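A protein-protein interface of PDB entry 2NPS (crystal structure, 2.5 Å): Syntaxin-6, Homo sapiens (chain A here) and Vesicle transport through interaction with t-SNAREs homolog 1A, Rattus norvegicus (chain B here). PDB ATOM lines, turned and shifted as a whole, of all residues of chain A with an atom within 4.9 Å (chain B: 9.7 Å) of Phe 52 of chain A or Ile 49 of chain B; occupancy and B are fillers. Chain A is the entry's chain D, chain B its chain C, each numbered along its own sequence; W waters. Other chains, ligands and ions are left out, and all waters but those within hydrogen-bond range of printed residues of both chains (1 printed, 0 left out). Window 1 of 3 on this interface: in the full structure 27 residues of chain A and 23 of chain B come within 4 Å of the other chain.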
ATOM      1  N   GLN A  45     -13.092   4.986 -28.008  1.00  0.00           N
ATOM      2  CA  GLN A  45     -11.906   4.956 -27.182  1.00  0.00           C
ATOM      3  C   GLN A  45     -12.279   4.489 -25.786  1.00  0.00           C
ATOM      4  O   GLN A  45     -11.502   3.821 -25.121  1.00  0.00           O
ATOM      5  CB  GLN A  45     -11.255   6.330 -27.167  1.00  0.00           C
ATOM      6  CG  GLN A  45     -10.462   6.589 -28.431  1.00  0.00           C
ATOM      7  CD  GLN A  45      -9.753   7.921 -28.427  1.00  0.00           C
ATOM      8  OE1 GLN A  45      -9.384   8.435 -27.377  1.00  0.00           O
ATOM      9  NE2 GLN A  45      -9.535   8.479 -29.611  1.00  0.00           N
ATOM     10  N   MET A  48     -12.024   0.963 -26.056  1.00  0.00           N
ATOM     11  CA  MET A  48     -10.604   0.683 -26.179  1.00  0.00           C
ATOM     12  C   MET A  48      -9.835   0.881 -24.867  1.00  0.00           C
ATOM     13  O   MET A  48      -8.861   0.184 -24.608  1.00  0.00           O
ATOM     14  CB  MET A  48     -10.030   1.577 -27.277  1.00  0.00           C
ATOM     15  CG  MET A  48      -8.718   1.132 -27.878  1.00  0.00           C
ATOM     16  SD  MET A  48      -8.077   2.403 -28.993  1.00  0.00           S
ATOM     17  CE  MET A  48      -9.308   2.380 -30.252  1.00  0.00           C
ATOM     18  N   LEU A  49     -10.280   1.810 -24.029  1.00  0.00           N
ATOM     19  CA  LEU A  49      -9.594   2.063 -22.759  1.00  0.00           C
ATOM     20  C   LEU A  49      -9.954   1.057 -21.682  1.00  0.00           C
ATOM     21  O   LEU A  49      -9.152   0.769 -20.779  1.00  0.00           O
ATOM     22  CB  LEU A  49      -9.910   3.467 -22.248  1.00  0.00           C
ATOM     23  CG  LEU A  49      -9.440   4.615 -23.136  1.00  0.00           C
ATOM     24  CD1 LEU A  49     -10.043   5.902 -22.642  1.00  0.00           C
ATOM     25  CD2 LEU A  49      -7.922   4.685 -23.164  1.00  0.00           C
ATOM     26  N   GLU A  50     -11.170   0.534 -21.765  1.00  0.00           N
ATOM     27  CA  GLU A  50     -11.582  -0.437 -20.789  1.00  0.00           C
ATOM     28  C   GLU A  50     -10.867  -1.727 -21.135  1.00  0.00           C
ATOM     29  O   GLU A  50     -10.527  -2.521 -20.263  1.00  0.00           O
ATOM     30  CB  GLU A  50     -13.086  -0.632 -20.808  1.00  0.00           C
ATOM     31  CG  GLU A  50     -13.535  -1.305 -19.546  1.00  0.00           C
ATOM     32  CD  GLU A  50     -14.844  -2.020 -19.690  1.00  0.00           C
ATOM     33  OE1 GLU A  50     -15.882  -1.331 -19.734  1.00  0.00           O
ATOM     34  OE2 GLU A  50     -14.825  -3.267 -19.766  1.00  0.00           O
ATOM     35  N   ASP A  51     -10.620  -1.915 -22.424  1.00  0.00           N
ATOM     36  CA  ASP A  51      -9.908  -3.095 -22.894  1.00  0.00           C
ATOM     37  C   ASP A  51      -8.473  -3.016 -22.391  1.00  0.00           C
ATOM     38  O   ASP A  51      -7.959  -3.974 -21.810  1.00  0.00           O
ATOM     39  CB  ASP A  51      -9.920  -3.178 -24.432  1.00  0.00           C
ATOM     40  CG  ASP A  51     -11.272  -3.658 -24.994  1.00  0.00           C
ATOM     41  OD1 ASP A  51     -11.424  -3.741 -26.238  1.00  0.00           O
ATOM     42  OD2 ASP A  51     -12.192  -3.961 -24.196  1.00  0.00           O
ATOM     43  N   PHE A  52      -7.842  -1.863 -22.607  1.00  0.00           N
ATOM     44  CA  PHE A  52      -6.470  -1.613 -22.155  1.00  0.00           C
ATOM     45  C   PHE A  52      -6.412  -1.817 -20.635  1.00  0.00           C
ATOM     46  O   PHE A  52      -5.482  -2.408 -20.099  1.00  0.00           O
ATOM     47  CB  PHE A  52      -6.058  -0.177 -22.523  1.00  0.00           C
ATOM     48  CG  PHE A  52      -4.596   0.116 -22.313  1.00  0.00           C
ATOM     49  CD1 PHE A  52      -4.119   1.411 -22.437  1.00  0.00           C
ATOM     50  CD2 PHE A  52      -3.695  -0.891 -22.006  1.00  0.00           C
ATOM     51  CE1 PHE A  52      -2.764   1.702 -22.263  1.00  0.00           C
ATOM     52  CE2 PHE A  52      -2.339  -0.613 -21.828  1.00  0.00           C
ATOM     53  CZ  PHE A  52      -1.870   0.691 -21.957  1.00  0.00           C
ATOM     54  N   SER A  53      -7.421  -1.330 -19.943  1.00  0.00           N
ATOM     55  CA  SER A  53      -7.450  -1.515 -18.521  1.00  0.00           C
ATOM     56  C   SER A  53      -7.426  -2.993 -18.154  1.00  0.00           C
ATOM     57  O   SER A  53      -6.703  -3.390 -17.251  1.00  0.00           O
ATOM     58  CB  SER A  53      -8.693  -0.875 -17.934  1.00  0.00           C
ATOM     59  OG  SER A  53      -8.745  -1.161 -16.556  1.00  0.00           O
ATOM     60  N   HIS A  54      -8.209  -3.815 -18.851  1.00  0.00           N
ATOM     61  CA  HIS A  54      -8.253  -5.241 -18.527  1.00  0.00           C
ATOM     62  C   HIS A  54      -6.988  -5.999 -18.863  1.00  0.00           C
ATOM     63  O   HIS A  54      -6.596  -6.925 -18.153  1.00  0.00           O
ATOM     64  CB  HIS A  54      -9.466  -5.904 -19.186  1.00  0.00           C
ATOM     65  CG  HIS A  54     -10.758  -5.526 -18.532  1.00  0.00           C
ATOM     66  ND1 HIS A  54     -10.991  -5.740 -17.189  1.00  0.00           N
ATOM     67  CD2 HIS A  54     -11.830  -4.835 -18.992  1.00  0.00           C
ATOM     68  CE1 HIS A  54     -12.144  -5.189 -16.848  1.00  0.00           C
ATOM     69  NE2 HIS A  54     -12.672  -4.632 -17.923  1.00  0.00           N
ATOM     70  N   GLU A  55      -6.335  -5.594 -19.937  1.00  0.00           N
ATOM     71  CA  GLU A  55      -5.101  -6.227 -20.323  1.00  0.00           C
ATOM     72  C   GLU A  55      -4.052  -5.880 -19.262  1.00  0.00           C
ATOM     73  O   GLU A  55      -3.241  -6.725 -18.884  1.00  0.00           O
ATOM     74  CB  GLU A  55      -4.699  -5.721 -21.690  1.00  0.00           C
ATOM     75  CG  GLU A  55      -5.846  -5.824 -22.668  1.00  0.00           C
ATOM     76  CD  GLU A  55      -5.557  -5.141 -23.975  1.00  0.00           C
ATOM     77  OE1 GLU A  55      -6.493  -5.034 -24.801  1.00  0.00           O
ATOM     78  OE2 GLU A  55      -4.394  -4.716 -24.173  1.00  0.00           O
ATOM     79  N   LEU A  56      -4.080  -4.639 -18.770  1.00  0.00           N
ATOM     80  CA  LEU A  56      -3.158  -4.207 -17.732  1.00  0.00           C
ATOM     81  C   LEU A  56      -3.340  -5.107 -16.534  1.00  0.00           C
ATOM     82  O   LEU A  56      -2.374  -5.637 -16.022  1.00  0.00           O
ATOM     83  CB  LEU A  56      -3.436  -2.760 -17.315  1.00  0.00           C
ATOM     84  CG  LEU A  56      -2.719  -1.595 -17.999  1.00  0.00           C
ATOM     85  CD1 LEU A  56      -3.185  -0.272 -17.420  1.00  0.00           C
ATOM     86  CD2 LEU A  56      -1.226  -1.729 -17.793  1.00  0.00           C
ATOM     87  N   ASN B  41      -6.318  15.453 -32.750  1.00  0.00           N
ATOM     88  CA  ASN B  41      -5.797  15.160 -31.415  1.00  0.00           C
ATOM     89  C   ASN B  41      -6.213  13.771 -30.924  1.00  0.00           C
ATOM     90  O   ASN B  41      -5.382  12.993 -30.461  1.00  0.00           O
ATOM     91  CB  ASN B  41      -6.298  16.260 -30.462  1.00  0.00           C
ATOM     92  CG  ASN B  41      -5.712  16.171 -29.062  1.00  0.00           C
ATOM     93  OD1 ASN B  41      -5.253  17.176 -28.511  1.00  0.00           O
ATOM     94  ND2 ASN B  41      -5.754  14.982 -28.465  1.00  0.00           N
ATOM     95  N   LEU B  42      -7.500  13.464 -31.039  1.00  0.00           N
ATOM     96  CA  LEU B  42      -8.034  12.174 -30.607  1.00  0.00           C
ATOM     97  C   LEU B  42      -7.470  11.001 -31.392  1.00  0.00           C
ATOM     98  O   LEU B  42      -7.228   9.935 -30.843  1.00  0.00           O
ATOM     99  CB  LEU B  42      -9.556  12.179 -30.716  1.00  0.00           C
ATOM    100  CG  LEU B  42     -10.258  13.086 -29.706  1.00  0.00           C
ATOM    101  CD1 LEU B  42     -11.692  13.355 -30.107  1.00  0.00           C
ATOM    102  CD2 LEU B  42     -10.180  12.437 -28.337  1.00  0.00           C
ATOM    103  N   SER B  43      -7.263  11.197 -32.685  1.00  0.00           N
ATOM    104  CA  SER B  43      -6.703  10.152 -33.521  1.00  0.00           C
ATOM    105  C   SER B  43      -5.299   9.852 -33.027  1.00  0.00           C
ATOM    106  O   SER B  43      -4.887   8.701 -32.929  1.00  0.00           O
ATOM    107  CB  SER B  43      -6.652  10.615 -34.974  1.00  0.00           C
ATOM    108  N   HIS B  44      -4.577  10.910 -32.703  1.00  0.00           N
ATOM    109  CA  HIS B  44      -3.215  10.803 -32.226  1.00  0.00           C
ATOM    110  C   HIS B  44      -3.168  10.020 -30.916  1.00  0.00           C
ATOM    111  O   HIS B  44      -2.313   9.157 -30.715  1.00  0.00           O
ATOM    112  CB  HIS B  44      -2.643  12.203 -32.017  1.00  0.00           C
ATOM    113  CG  HIS B  44      -1.152  12.268 -32.122  1.00  0.00           C
ATOM    114  ND1 HIS B  44      -0.495  12.343 -33.334  1.00  0.00           N
ATOM    115  CD2 HIS B  44      -0.188  12.234 -31.169  1.00  0.00           C
ATOM    116  CE1 HIS B  44       0.811  12.351 -33.123  1.00  0.00           C
ATOM    117  NE2 HIS B  44       1.023  12.285 -31.818  1.00  0.00           N
ATOM    118  N   ASP B  45      -4.105  10.316 -30.026  1.00  0.00           N
ATOM    119  CA  ASP B  45      -4.164   9.634 -28.742  1.00  0.00           C
ATOM    120  C   ASP B  45      -4.554   8.185 -28.952  1.00  0.00           C
ATOM    121  O   ASP B  45      -3.942   7.285 -28.382  1.00  0.00           O
ATOM    122  CB  ASP B  45      -5.156  10.349 -27.827  1.00  0.00           C
ATOM    123  CG  ASP B  45      -4.731  11.774 -27.526  1.00  0.00           C
ATOM    124  OD1 ASP B  45      -5.595  12.593 -27.144  1.00  0.00           O
ATOM    125  OD2 ASP B  45      -3.518  12.071 -27.669  1.00  0.00           O
ATOM    126  N   ARG B  46      -5.556   7.969 -29.796  1.00  0.00           N
ATOM    127  CA  ARG B  46      -6.010   6.620 -30.114  1.00  0.00           C
ATOM    128  C   ARG B  46      -4.838   5.799 -30.643  1.00  0.00           C
ATOM    129  O   ARG B  46      -4.760   4.594 -30.409  1.00  0.00           O
ATOM    130  CB  ARG B  46      -7.116   6.665 -31.171  1.00  0.00           C
ATOM    131  CG  ARG B  46      -7.562   5.303 -31.674  1.00  0.00           C
ATOM    132  CD  ARG B  46      -8.460   5.435 -32.911  1.00  0.00           C
ATOM    133  NE  ARG B  46      -9.095   4.169 -33.271  1.00  0.00           N
ATOM    134  CZ  ARG B  46     -10.358   3.861 -33.002  1.00  0.00           C
ATOM    135  NH1 ARG B  46     -10.846   2.680 -33.360  1.00  0.00           N
ATOM    136  NH2 ARG B  46     -11.139   4.737 -32.389  1.00  0.00           N
ATOM    137  N   GLU B  47      -3.925   6.462 -31.350  1.00  0.00           N
ATOM    138  CA  GLU B  47      -2.764   5.783 -31.892  1.00  0.00           C
ATOM    139  C   GLU B  47      -1.831   5.423 -30.741  1.00  0.00           C
ATOM    140  O   GLU B  47      -1.382   4.286 -30.640  1.00  0.00           O
ATOM    141  CB  GLU B  47      -2.058   6.671 -32.931  1.00  0.00           C
ATOM    142  CG  GLU B  47      -1.119   5.902 -33.890  1.00  0.00           C
ATOM    143  CD  GLU B  47      -1.045   6.498 -35.318  1.00  0.00           C
ATOM    144  OE1 GLU B  47      -0.443   5.846 -36.213  1.00  0.00           O
ATOM    145  OE2 GLU B  47      -1.583   7.606 -35.553  1.00  0.00           O
ATOM    146  N   ARG B  48      -1.567   6.377 -29.855  1.00  0.00           N
ATOM    147  CA  ARG B  48      -0.694   6.139 -28.710  1.00  0.00           C
ATOM    148  C   ARG B  48      -1.235   5.053 -27.757  1.00  0.00           C
ATOM    149  O   ARG B  48      -0.474   4.269 -27.199  1.00  0.00           O
ATOM    150  CB  ARG B  48      -0.479   7.449 -27.971  1.00  0.00           C
ATOM    151  CG  ARG B  48       0.031   8.549 -28.872  1.00  0.00           C
ATOM    152  CD  ARG B  48      -0.085   9.894 -28.207  1.00  0.00           C
ATOM    153  NE  ARG B  48       0.736   9.971 -27.006  1.00  0.00           N
ATOM    154  CZ  ARG B  48       0.644  10.934 -26.101  1.00  0.00           C
ATOM    155  NH1 ARG B  48       1.444  10.922 -25.044  1.00  0.00           N
ATOM    156  NH2 ARG B  48      -0.254  11.900 -26.246  1.00  0.00           N
ATOM    157  N   ILE B  49      -2.547   4.996 -27.578  1.00  0.00           N
ATOM    158  CA  ILE B  49      -3.136   3.964 -26.728  1.00  0.00           C
ATOM    159  C   ILE B  49      -2.936   2.592 -27.388  1.00  0.00           C
ATOM    160  O   ILE B  49      -2.623   1.617 -26.712  1.00  0.00           O
ATOM    161  CB  ILE B  49      -4.664   4.188 -26.521  1.00  0.00           C
ATOM    162  CG1 ILE B  49      -4.919   5.499 -25.772  1.00  0.00           C
ATOM    163  CG2 ILE B  49      -5.274   3.009 -25.774  1.00  0.00           C
ATOM    164  CD1 ILE B  49      -6.336   6.021 -25.946  1.00  0.00           C
ATOM    165  N   GLN B  50      -3.129   2.509 -28.703  1.00  0.00           N
ATOM    166  CA  GLN B  50      -2.957   1.232 -29.395  1.00  0.00           C
ATOM    167  C   GLN B  50      -1.493   0.830 -29.354  1.00  0.00           C
ATOM    168  O   GLN B  50      -1.167  -0.343 -29.190  1.00  0.00           O
ATOM    169  CB  GLN B  50      -3.433   1.301 -30.850  1.00  0.00           C
ATOM    170  CG  GLN B  50      -4.938   1.547 -31.065  1.00  0.00           C
ATOM    171  CD  GLN B  50      -5.856   0.516 -30.396  1.00  0.00           C
ATOM    172  OE1 GLN B  50      -6.780  -0.021 -31.019  1.00  0.00           O
ATOM    173  NE2 GLN B  50      -5.614   0.251 -29.129  1.00  0.00           N
ATOM    174  N   ARG B  51      -0.605   1.800 -29.490  1.00  0.00           N
ATOM    175  CA  ARG B  51       0.807   1.503 -29.421  1.00  0.00           C
ATOM    176  C   ARG B  51       1.158   0.928 -28.046  1.00  0.00           C
ATOM    177  O   ARG B  51       1.945  -0.009 -27.946  1.00  0.00           O
ATOM    178  CB  ARG B  51       1.611   2.766 -29.675  1.00  0.00           C
ATOM    179  CG  ARG B  51       1.963   2.982 -31.118  1.00  0.00           C
ATOM    180  CD  ARG B  51       2.413   4.401 -31.353  1.00  0.00           C
ATOM    181  NE  ARG B  51       3.339   4.856 -30.317  1.00  0.00           N
ATOM    182  CZ  ARG B  51       3.622   6.136 -30.093  1.00  0.00           C
ATOM    183  NH1 ARG B  51       3.049   7.070 -30.837  1.00  0.00           N
ATOM    184  NH2 ARG B  51       4.457   6.484 -29.123  1.00  0.00           N
ATOM    185  N   ALA B  52       0.558   1.485 -26.994  1.00  0.00           N
ATOM    186  CA  ALA B  52       0.797   1.049 -25.614  1.00  0.00           C
ATOM    187  C   ALA B  52       0.203  -0.314 -25.342  1.00  0.00           C
ATOM    188  O   ALA B  52       0.790  -1.119 -24.633  1.00  0.00           O
ATOM    189  CB  ALA B  52       0.224   2.057 -24.643  1.00  0.00           C
ATOM    190  N   ARG B  53      -0.976  -0.557 -25.900  1.00  0.00           N
ATOM    191  CA  ARG B  53      -1.634  -1.846 -25.748  1.00  0.00           C
ATOM    192  C   ARG B  53      -0.737  -2.869 -26.395  1.00  0.00           C
ATOM    193  O   ARG B  53      -0.603  -3.983 -25.909  1.00  0.00           O
ATOM    194  CB  ARG B  53      -2.978  -1.853 -26.457  1.00  0.00           C
ATOM    195  CG  ARG B  53      -4.007  -0.991 -25.789  1.00  0.00           C
ATOM    196  CD  ARG B  53      -5.318  -1.080 -26.524  1.00  0.00           C
ATOM    197  NE  ARG B  53      -5.877  -2.420 -26.452  1.00  0.00           N
ATOM    198  CZ  ARG B  53      -6.961  -2.809 -27.112  1.00  0.00           C
ATOM    199  NH1 ARG B  53      -7.399  -4.045 -26.975  1.00  0.00           N
ATOM    200  NH2 ARG B  53      -7.600  -1.968 -27.918  1.00  0.00           N
ATOM    201  N   GLU B  54      -0.115  -2.472 -27.497  1.00  0.00           N
ATOM    202  CA  GLU B  54       0.783  -3.342 -28.229  1.00  0.00           C
ATOM    203  C   GLU B  54       2.012  -3.659 -27.399  1.00  0.00           C
ATOM    204  O   GLU B  54       2.394  -4.824 -27.273  1.00  0.00           O
ATOM    205  CB  GLU B  54       1.199  -2.674 -29.539  1.00  0.00           C
ATOM    206  CG  GLU B  54       2.169  -3.498 -30.380  1.00  0.00           C
ATOM    207  N   ARG B  55       2.615  -2.616 -26.826  1.00  0.00           N
ATOM    208  CA  ARG B  55       3.825  -2.736 -26.002  1.00  0.00           C
ATOM    209  C   ARG B  55       3.554  -3.587 -24.764  1.00  0.00           C
ATOM    210  O   ARG B  55       4.447  -4.199 -24.197  1.00  0.00           O
ATOM    211  CB  ARG B  55       4.289  -1.350 -25.575  1.00  0.00           C
ATOM    212  CG  ARG B  55       5.723  -1.274 -25.110  1.00  0.00           C
ATOM    213  CD  ARG B  55       6.688  -1.220 -26.299  1.00  0.00           C
ATOM    214  NE  ARG B  55       8.082  -1.053 -25.885  1.00  0.00           N
ATOM    215  CZ  ARG B  55       9.052  -1.919 -26.164  1.00  0.00           C
ATOM    216  NH1 ARG B  55       8.785  -3.021 -26.864  1.00  0.00           N
ATOM    217  NH2 ARG B  55      10.289  -1.690 -25.738  1.00  0.00           N
ATOM    218  N   LEU B  56       2.300  -3.620 -24.351  1.00  0.00           N
ATOM    219  CA  LEU B  56       1.907  -4.391 -23.197  1.00  0.00           C
ATOM    220  C   LEU B  56       1.905  -5.859 -23.575  1.00  0.00           C
ATOM    221  O   LEU B  56       2.321  -6.713 -22.792  1.00  0.00           O
ATOM    222  CB  LEU B  56       0.513  -3.981 -22.766  1.00  0.00           C
ATOM    223  CG  LEU B  56       0.259  -3.675 -21.301  1.00  0.00           C
ATOM    224  CD1 LEU B  56      -1.111  -4.224 -20.965  1.00  0.00           C
ATOM    225  CD2 LEU B  56       1.328  -4.275 -20.410  1.00  0.00           C
ATOM    226  N   ARG B  57       1.423  -6.158 -24.774  1.00  0.00           N
ATOM    227  CA  ARG B  57       1.389  -7.538 -25.228  1.00  0.00           C
ATOM    228  C   ARG B  57       2.797  -8.082 -25.323  1.00  0.00           C
ATOM    229  O   ARG B  57       3.027  -9.263 -25.073  1.00  0.00           O
ATOM    230  CB  ARG B  57       0.687  -7.653 -26.579  1.00  0.00           C
ATOM    231  CG  ARG B  57      -0.800  -7.855 -26.454  1.00  0.00           C
ATOM    232  CD  ARG B  57      -1.500  -7.810 -27.803  1.00  0.00           C
ATOM    233  NE  ARG B  57      -1.751  -6.445 -28.262  1.00  0.00           N
ATOM    234  CZ  ARG B  57      -2.949  -5.865 -28.273  1.00  0.00           C
ATOM    235  NH1 ARG B  57      -3.065  -4.620 -28.709  1.00  0.00           N
ATOM    236  NH2 ARG B  57      -4.031  -6.528 -27.863  1.00  0.00           N
ATOM    237  N   THR B  59       5.194  -7.142 -23.402  1.00  0.00           N
ATOM    238  CA  THR B  59       5.605  -7.333 -22.013  1.00  0.00           C
ATOM    239  C   THR B  59       5.068  -8.698 -21.585  1.00  0.00           C
ATOM    240  O   THR B  59       5.706  -9.423 -20.833  1.00  0.00           O
ATOM    241  CB  THR B  59       5.038  -6.234 -21.086  1.00  0.00           C
ATOM    242  OG1 THR B  59       5.415  -4.948 -21.592  1.00  0.00           O
ATOM    243  CG2 THR B  59       5.581  -6.389 -19.679  1.00  0.00           C
ATOM    244  N   ASP B  60       3.894  -9.046 -22.096  1.00  0.00           N
ATOM    245  CA  ASP B  60       3.277 -10.334 -21.812  1.00  0.00           C
ATOM    246  C   ASP B  60       4.135 -11.448 -22.396  1.00  0.00           C
ATOM    247  O   ASP B  60       4.425 -12.434 -21.732  1.00  0.00           O
ATOM    248  CB  ASP B  60       1.884 -10.394 -22.424  1.00  0.00           C
ATOM    249  CG  ASP B  60       0.831  -9.800 -21.524  1.00  0.00           C
ATOM    250  OD1 ASP B  60      -0.293  -9.549 -22.001  1.00  0.00           O
ATOM    251  OD2 ASP B  60       1.115  -9.586 -20.330  1.00  0.00           O
HETATM  252  O   HOH W   1      -9.838  -3.277 -28.987  1.00  0.00           O
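The backbone carbonyl oxygen (O) of Leu 42 of chain B sits at hydrogen-bond distance from the side-chain amide nitrogen (NE2) of Gln 45 of chain A.
The guanidinium group (NH1) of Arg 53 of chain B lies within salt-bridge range of the side-chain carboxylate (OE1) of Glu 55 of chain A, at 2.6 Å.
The side-chain sulfur of Met 48 of chain A sits close to the side-chain amide nitrogen of Gln 50 of chain B.
Among the printed residues, pairs that only touch across the chains: Gln 45 of chain A with Arg 46 of chain B, Met 48 of chain A with Arg 46 of chain B, Met 48 of chain A with Arg 53 of chain B, Leu 49 of chain A with Ile 49 of chain B, Asp 51 of chain A with Arg 53 of chain B, Phe 52 of chain A with Ile 49 of chain B, Phe 52 of chain A with Ala 52 of chain B, Phe 52 of chain A with Arg 53 of chain B, Phe 52 of chain A with Leu 56 of chain B, Glu 55 of chain A with Leu 56 of chain B and Leu 56 of chain A with Leu 56 of chain B.
Water W1 bridges the guanidinium group (NH2) of Arg 53 of chain B (2.8 Å) and the side-chain carboxylate (OD1) of Asp 51 of chain A (3.2 Å).
Phe 52 of chain A touches just these residues of chain B: Ile 49 (3.9 Å), Ala 52 (3.7 Å), Arg 53 (3.7 Å) and Leu 56 (3.9 Å).
Glu 55 of chain A touches just these residues of chain B: Arg 53 and Leu 56.
Of the printed residues of chain A, Gln 50 of chain B touches Met 48 (3.2 Å).
Of the printed residues of chain B, Met 48 of chain A touches Arg 46 (3.3 Å), Gln 50 (3.2 Å) and Arg 53 (3.3 Å).
The nearest residue of chain B that does not touch Phe 52 of chain A is Arg 48 of chain B (6.0 Å).
The guanidinium group (NH2) of Arg 53 of chain B sits close to the side-chain amide nitrogen (NE2) of Gln 50 of chain B (3.2 Å).
Among the printed residues, Asp or Glu carboxylates within 4 Å of a Lys or Arg side-chain nitrogen of the other chain: Glu 55 of chain A with Arg 53 of chain B (2.6 Å).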
